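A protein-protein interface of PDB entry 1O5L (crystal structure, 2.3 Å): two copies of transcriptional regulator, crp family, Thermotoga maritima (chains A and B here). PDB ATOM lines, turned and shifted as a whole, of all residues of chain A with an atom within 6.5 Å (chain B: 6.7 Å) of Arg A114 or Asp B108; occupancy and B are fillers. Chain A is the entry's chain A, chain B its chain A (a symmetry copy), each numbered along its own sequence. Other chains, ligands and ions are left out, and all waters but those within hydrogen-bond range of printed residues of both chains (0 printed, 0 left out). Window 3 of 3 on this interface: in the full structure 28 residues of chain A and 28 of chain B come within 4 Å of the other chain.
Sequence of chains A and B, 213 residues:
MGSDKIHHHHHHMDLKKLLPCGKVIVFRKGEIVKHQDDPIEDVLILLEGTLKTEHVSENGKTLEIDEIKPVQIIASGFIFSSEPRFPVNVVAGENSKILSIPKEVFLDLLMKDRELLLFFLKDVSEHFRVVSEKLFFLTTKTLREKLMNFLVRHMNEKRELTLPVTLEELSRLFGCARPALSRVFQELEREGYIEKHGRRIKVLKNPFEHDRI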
ATOM      1  N   LEU A 109      30.193  -1.093  32.478  1.00  0.00           N
ATOM      2  CA  LEU A 109      30.082  -1.590  31.105  1.00  0.00           C
ATOM      3  C   LEU A 109      28.950  -0.905  30.308  1.00  0.00           C
ATOM      4  O   LEU A 109      29.136  -0.554  29.145  1.00  0.00           O
ATOM      5  CB  LEU A 109      29.851  -3.105  31.093  1.00  0.00           C
ATOM      6  CG  LEU A 109      31.015  -3.981  31.531  1.00  0.00           C
ATOM      7  CD1 LEU A 109      30.581  -5.419  31.710  1.00  0.00           C
ATOM      8  CD2 LEU A 109      32.215  -3.904  30.562  1.00  0.00           C
ATOM      9  N   LEU A 110      27.786  -0.745  30.946  1.00  0.00           N
ATOM     10  CA  LEU A 110      26.659  -0.028  30.370  1.00  0.00           C
ATOM     11  C   LEU A 110      27.043   1.387  29.972  1.00  0.00           C
ATOM     12  O   LEU A 110      26.588   1.892  28.929  1.00  0.00           O
ATOM     13  CB  LEU A 110      25.499   0.059  31.383  1.00  0.00           C
ATOM     14  CG  LEU A 110      24.746  -1.235  31.708  1.00  0.00           C
ATOM     15  CD1 LEU A 110      23.603  -1.007  32.684  1.00  0.00           C
ATOM     16  CD2 LEU A 110      24.203  -1.858  30.426  1.00  0.00           C
ATOM     17  N   MET A 111      27.850   2.048  30.814  1.00  0.00           N
ATOM     18  CA  MET A 111      28.220   3.449  30.567  1.00  0.00           C
ATOM     19  C   MET A 111      29.208   3.582  29.410  1.00  0.00           C
ATOM     20  O   MET A 111      29.295   4.649  28.785  1.00  0.00           O
ATOM     21  CB  MET A 111      28.780   4.111  31.839  1.00  0.00           C
ATOM     22  CG  MET A 111      27.688   4.334  32.913  1.00  0.00           C
ATOM     23  SD  MET A 111      28.159   5.235  34.402  1.00  0.00           S
ATOM     24  CE  MET A 111      29.277   4.446  34.854  1.00  0.00           C
ATOM     25  N   LYS A 112      29.942   2.511  29.111  1.00  0.00           N
ATOM     26  CA  LYS A 112      31.002   2.580  28.099  1.00  0.00           C
ATOM     27  C   LYS A 112      30.639   1.995  26.730  1.00  0.00           C
ATOM     28  O   LYS A 112      31.399   2.204  25.759  1.00  0.00           O
ATOM     29  CB  LYS A 112      32.267   1.901  28.628  1.00  0.00           C
ATOM     30  N   ASP A 113      29.514   1.280  26.646  1.00  0.00           N
ATOM     31  CA  ASP A 113      29.109   0.542  25.445  1.00  0.00           C
ATOM     32  C   ASP A 113      27.607   0.784  25.145  1.00  0.00           C
ATOM     33  O   ASP A 113      26.726   0.312  25.861  1.00  0.00           O
ATOM     34  CB  ASP A 113      29.405  -0.950  25.666  1.00  0.00           C
ATOM     35  CG  ASP A 113      29.122  -1.823  24.459  1.00  0.00           C
ATOM     36  OD1 ASP A 113      28.449  -1.400  23.486  1.00  0.00           O
ATOM     37  OD2 ASP A 113      29.521  -3.005  24.415  1.00  0.00           O
ATOM     38  N   ARG A 114      27.342   1.529  24.079  1.00  0.00           N
ATOM     39  CA  ARG A 114      25.992   1.968  23.748  1.00  0.00           C
ATOM     40  C   ARG A 114      25.119   0.794  23.310  1.00  0.00           C
ATOM     41  O   ARG A 114      23.946   0.689  23.665  1.00  0.00           O
ATOM     42  CB  ARG A 114      26.055   3.014  22.605  1.00  0.00           C
ATOM     43  CG  ARG A 114      24.754   3.759  22.346  1.00  0.00           C
ATOM     44  CD  ARG A 114      24.836   4.634  21.116  1.00  0.00           C
ATOM     45  NE  ARG A 114      23.773   5.636  21.003  1.00  0.00           N
ATOM     46  CZ  ARG A 114      23.775   6.826  21.616  1.00  0.00           C
ATOM     47  NH1 ARG A 114      24.773   7.150  22.442  1.00  0.00           N
ATOM     48  NH2 ARG A 114      22.780   7.693  21.413  1.00  0.00           N
ATOM     49  N   GLU A 115      25.712  -0.082  22.523  1.00  0.00           N
ATOM     50  CA  GLU A 115      25.036  -1.251  21.996  1.00  0.00           C
ATOM     51  C   GLU A 115      24.561  -2.167  23.149  1.00  0.00           C
ATOM     52  O   GLU A 115      23.452  -2.697  23.105  1.00  0.00           O
ATOM     53  CB  GLU A 115      25.966  -1.917  20.947  1.00  0.00           C
ATOM     54  CG  GLU A 115      25.994  -3.427  20.931  1.00  0.00           C
ATOM     55  CD  GLU A 115      26.595  -4.022  19.666  1.00  0.00           C
ATOM     56  OE1 GLU A 115      27.615  -3.498  19.188  1.00  0.00           O
ATOM     57  OE2 GLU A 115      26.056  -5.024  19.153  1.00  0.00           O
ATOM     58  N   LEU A 116      25.376  -2.284  24.211  1.00  0.00           N
ATOM     59  CA  LEU A 116      25.012  -3.016  25.417  1.00  0.00           C
ATOM     60  C   LEU A 116      23.886  -2.334  26.199  1.00  0.00           C
ATOM     61  O   LEU A 116      22.911  -2.981  26.625  1.00  0.00           O
ATOM     62  CB  LEU A 116      26.240  -3.185  26.331  1.00  0.00           C
ATOM     63  CG  LEU A 116      26.046  -3.964  27.645  1.00  0.00           C
ATOM     64  CD1 LEU A 116      25.582  -5.425  27.386  1.00  0.00           C
ATOM     65  CD2 LEU A 116      27.317  -3.962  28.469  1.00  0.00           C
ATOM     66  N   LEU A 117      24.034  -1.025  26.398  1.00  0.00           N
ATOM     67  CA  LEU A 117      23.029  -0.229  27.099  1.00  0.00           C
ATOM     68  C   LEU A 117      21.660  -0.382  26.411  1.00  0.00           C
ATOM     69  O   LEU A 117      20.640  -0.644  27.061  1.00  0.00           O
ATOM     70  CB  LEU A 117      23.450   1.260  27.134  1.00  0.00           C
ATOM     71  CG  LEU A 117      22.452   2.210  27.825  1.00  0.00           C
ATOM     72  CD1 LEU A 117      22.098   1.754  29.244  1.00  0.00           C
ATOM     73  CD2 LEU A 117      23.018   3.624  27.870  1.00  0.00           C
ATOM     74  N   LEU A 118      21.660  -0.179  25.097  1.00  0.00           N
ATOM     75  CA  LEU A 118      20.460  -0.325  24.300  1.00  0.00           C
ATOM     76  C   LEU A 118      19.856  -1.725  24.393  1.00  0.00           C
ATOM     77  O   LEU A 118      18.651  -1.851  24.569  1.00  0.00           O
ATOM     78  CB  LEU A 118      20.734   0.021  22.843  1.00  0.00           C
ATOM     79  CG  LEU A 118      20.541   1.503  22.502  1.00  0.00           C
ATOM     80  CD1 LEU A 118      21.185   1.818  21.171  1.00  0.00           C
ATOM     81  CD2 LEU A 118      19.062   1.839  22.486  1.00  0.00           C
ATOM     82  N   PHE A 119      20.708  -2.752  24.272  1.00  0.00           N
ATOM     83  CA  PHE A 119      20.287  -4.134  24.425  1.00  0.00           C
ATOM     84  C   PHE A 119      19.595  -4.381  25.762  1.00  0.00           C
ATOM     85  O   PHE A 119      18.475  -4.892  25.782  1.00  0.00           O
ATOM     86  CB  PHE A 119      21.475  -5.079  24.282  1.00  0.00           C
ATOM     87  CG  PHE A 119      21.119  -6.521  24.502  1.00  0.00           C
ATOM     88  CD1 PHE A 119      21.150  -7.075  25.790  1.00  0.00           C
ATOM     89  CD2 PHE A 119      20.724  -7.323  23.436  1.00  0.00           C
ATOM     90  CE1 PHE A 119      20.786  -8.416  26.005  1.00  0.00           C
ATOM     91  CE2 PHE A 119      20.381  -8.674  23.639  1.00  0.00           C
ATOM     92  CZ  PHE A 119      20.417  -9.216  24.924  1.00  0.00           C
ATOM     93  N   LYS B 103      15.476  10.969  22.271  1.00  0.00           N
ATOM     94  CA  LYS B 103      15.909   9.682  22.788  1.00  0.00           C
ATOM     95  C   LYS B 103      17.438   9.484  22.749  1.00  0.00           C
ATOM     96  O   LYS B 103      18.012   8.931  23.680  1.00  0.00           O
ATOM     97  CB  LYS B 103      15.213   8.546  22.038  1.00  0.00           C
ATOM     98  CG  LYS B 103      14.250   7.761  22.896  1.00  0.00           C
ATOM     99  CD  LYS B 103      13.851   6.383  22.269  1.00  0.00           C
ATOM    100  CE  LYS B 103      12.403   6.354  21.855  1.00  0.00           C
ATOM    101  NZ  LYS B 103      12.049   5.033  21.252  1.00  0.00           N
ATOM    102  N   GLU B 104      18.060   9.887  21.640  1.00  0.00           N
ATOM    103  CA  GLU B 104      19.502   9.703  21.436  1.00  0.00           C
ATOM    104  C   GLU B 104      20.310  10.544  22.407  1.00  0.00           C
ATOM    105  O   GLU B 104      21.334  10.073  22.924  1.00  0.00           O
ATOM    106  CB  GLU B 104      19.938  10.041  19.996  1.00  0.00           C
ATOM    107  CG  GLU B 104      19.402   9.095  18.925  1.00  0.00           C
ATOM    108  CD  GLU B 104      19.758   7.616  19.156  1.00  0.00           C
ATOM    109  OE1 GLU B 104      20.852   7.328  19.685  1.00  0.00           O
ATOM    110  OE2 GLU B 104      18.940   6.731  18.802  1.00  0.00           O
ATOM    111  N   VAL B 105      19.854  11.778  22.631  1.00  0.00           N
ATOM    112  CA  VAL B 105      20.430  12.633  23.630  1.00  0.00           C
ATOM    113  C   VAL B 105      20.200  12.036  25.030  1.00  0.00           C
ATOM    114  O   VAL B 105      21.130  12.050  25.868  1.00  0.00           O
ATOM    115  CB  VAL B 105      19.876  14.058  23.536  1.00  0.00           C
ATOM    116  CG1 VAL B 105      20.415  14.925  24.664  1.00  0.00           C
ATOM    117  CG2 VAL B 105      20.215  14.693  22.175  1.00  0.00           C
ATOM    118  N   PHE B 106      18.994  11.513  25.307  1.00  0.00           N
ATOM    119  CA  PHE B 106      18.784  10.924  26.642  1.00  0.00           C
ATOM    120  C   PHE B 106      19.756   9.751  26.866  1.00  0.00           C
ATOM    121  O   PHE B 106      20.351   9.653  27.914  1.00  0.00           O
ATOM    122  CB  PHE B 106      17.333  10.502  26.888  1.00  0.00           C
ATOM    123  CG  PHE B 106      17.036  10.208  28.337  1.00  0.00           C
ATOM    124  CD1 PHE B 106      16.929  11.243  29.264  1.00  0.00           C
ATOM    125  CD2 PHE B 106      16.885   8.887  28.789  1.00  0.00           C
ATOM    126  CE1 PHE B 106      16.668  10.967  30.638  1.00  0.00           C
ATOM    127  CE2 PHE B 106      16.629   8.596  30.142  1.00  0.00           C
ATOM    128  CZ  PHE B 106      16.509   9.637  31.066  1.00  0.00           C
ATOM    129  N   LEU B 107      19.987   8.926  25.853  1.00  0.00           N
ATOM    130  CA  LEU B 107      21.006   7.860  25.965  1.00  0.00           C
ATOM    131  C   LEU B 107      22.413   8.383  26.272  1.00  0.00           C
ATOM    132  O   LEU B 107      23.125   7.773  27.064  1.00  0.00           O
ATOM    133  CB  LEU B 107      21.109   7.032  24.677  1.00  0.00           C
ATOM    134  CG  LEU B 107      20.133   5.899  24.440  1.00  0.00           C
ATOM    135  CD1 LEU B 107      20.325   5.426  23.009  1.00  0.00           C
ATOM    136  CD2 LEU B 107      20.304   4.729  25.418  1.00  0.00           C
ATOM    137  N   ASP B 108      22.812   9.473  25.600  1.00  0.00           N
ATOM    138  CA  ASP B 108      24.121  10.094  25.813  1.00  0.00           C
ATOM    139  C   ASP B 108      24.253  10.526  27.264  1.00  0.00           C
ATOM    140  O   ASP B 108      25.291  10.320  27.848  1.00  0.00           O
ATOM    141  CB  ASP B 108      24.354  11.332  24.915  1.00  0.00           C
ATOM    142  CG  ASP B 108      24.405  11.009  23.431  1.00  0.00           C
ATOM    143  OD1 ASP B 108      24.614   9.845  23.071  1.00  0.00           O
ATOM    144  OD2 ASP B 108      24.266  11.873  22.535  1.00  0.00           O
ATOM    145  N   LEU B 109      23.215  11.152  27.813  1.00  0.00           N
ATOM    146  CA  LEU B 109      23.196  11.586  29.212  1.00  0.00           C
ATOM    147  C   LEU B 109      23.337  10.411  30.206  1.00  0.00           C
ATOM    148  O   LEU B 109      24.071  10.514  31.186  1.00  0.00           O
ATOM    149  CB  LEU B 109      21.904  12.348  29.527  1.00  0.00           C
ATOM    150  CG  LEU B 109      21.743  13.720  28.889  1.00  0.00           C
ATOM    151  CD1 LEU B 109      20.340  14.249  29.075  1.00  0.00           C
ATOM    152  CD2 LEU B 109      22.772  14.743  29.416  1.00  0.00           C
ATOM    153  N   LEU B 110      22.614   9.319  29.943  1.00  0.00           N
ATOM    154  CA  LEU B 110      22.715   8.094  30.723  1.00  0.00           C
ATOM    155  C   LEU B 110      24.142   7.575  30.760  1.00  0.00           C
ATOM    156  O   LEU B 110      24.600   7.071  31.803  1.00  0.00           O
ATOM    157  CB  LEU B 110      21.821   6.993  30.117  1.00  0.00           C
ATOM    158  CG  LEU B 110      20.304   7.165  30.242  1.00  0.00           C
ATOM    159  CD1 LEU B 110      19.540   5.994  29.646  1.00  0.00           C
ATOM    160  CD2 LEU B 110      19.919   7.329  31.710  1.00  0.00           C
ATOM    161  N   MET B 111      24.841   7.657  29.619  1.00  0.00           N
ATOM    162  CA  MET B 111      26.202   7.112  29.523  1.00  0.00           C
ATOM    163  C   MET B 111      27.215   7.966  30.283  1.00  0.00           C
ATOM    164  O   MET B 111      28.279   7.469  30.679  1.00  0.00           O
ATOM    165  CB  MET B 111      26.631   6.939  28.054  1.00  0.00           C
ATOM    166  CG  MET B 111      25.861   5.795  27.350  1.00  0.00           C
ATOM    167  SD  MET B 111      26.357   5.372  25.669  1.00  0.00           S
ATOM    168  CE  MET B 111      26.233   6.652  25.019  1.00  0.00           C
ATOM    169  N   LYS B 112      26.892   9.242  30.500  1.00  0.00           N
ATOM    170  CA  LYS B 112      27.849  10.170  31.111  1.00  0.00           C
ATOM    171  C   LYS B 112      27.621  10.461  32.599  1.00  0.00           C
ATOM    172  O   LYS B 112      28.506  11.066  33.241  1.00  0.00           O
ATOM    173  CB  LYS B 112      27.869  11.484  30.327  1.00  0.00           C
ATOM    174  N   ASP B 113      26.468  10.052  33.134  1.00  0.00           N
ATOM    175  CA  ASP B 113      26.045  10.380  34.499  1.00  0.00           C
ATOM    176  C   ASP B 113      25.486   9.120  35.209  1.00  0.00           C
ATOM    177  O   ASP B 113      24.409   8.626  34.882  1.00  0.00           O
ATOM    178  CB  ASP B 113      24.993  11.499  34.428  1.00  0.00           C
ATOM    179  CG  ASP B 113      24.537  12.007  35.782  1.00  0.00           C
ATOM    180  OD1 ASP B 113      24.788  11.375  36.839  1.00  0.00           O
ATOM    181  OD2 ASP B 113      23.862  13.053  35.881  1.00  0.00           O
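Met B111 touches its own counterpart, Met A111.
5 positions are printed for both chains.
Met A111 touches Met B111.
Leu B107 touches Arg A114 (CD1 to NH2, 3.7 Å).
Arg A114 touches Met B111.
Leu A117 touches Leu B107 (CD2 to CD2, 3.8 Å).
Leu A117 touches Met B111 (CD2 to CG, 3.6 Å).
Leu B107 touches Leu A118 (CD1 to CD2, 3.8 Å).
The guanidinium group of Arg A114 lies within salt-bridge range of the side-chain carboxylate of Asp B108 (2.8 Å).
The guanidinium group (NH2) of Arg A114 lies within salt-bridge range of the side-chain carboxylate (OE1) of Glu B104, at 2.6 Å.
Of the 11 printed residues of chain B, 4 touch a printed residue of chain A.
Printed residues of chain B that touch a printed residue of chain A: Glu B104, Leu B107, Asp B108 and Met B111.
Hydrophobic or aromatic side chains of chain B that line the printed part of chain A: Leu B107 and Met B111.
Printed residues of chain A that touch a printed residue of chain B: Met A111, Arg A114, Leu A117 and Leu A118.
Among the printed residues, Asp or Glu carboxylates within 4 Å of a Lys or Arg side-chain nitrogen of the other chain: Arg A114 with Glu B104 (2.6 Å) and Arg A114 with Asp B108 (2.8 Å).
Of the printed residues of chain B, Met A111 touches Met B111 (3.5 Å).
Of the printed residues of chain B, Arg A114 touches Glu B104 (2.6 Å), Leu B107 (3.7 Å), Asp B108 (2.8 Å) and Met B111 (3.0 Å).
Printed residues of chain B within 4 Å of Leu A117: Leu B107 (3.8 Å) and Met B111 (3.6 Å).
Phe A119 touches none of the printed residues of chain B.
Printed residues of chain A within 4 Å of Glu B104: Arg A114 (2.6 Å).
Printed residues of chain A within 4 Å of Leu B107: Arg A114 (3.7 Å), Leu A117 (3.8 Å) and Leu A118 (3.8 Å).
Asp B108 touches one residue of chain A.
Of the printed residues of chain A, Met B111 touches Met A111, Arg A114 and Leu A117.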
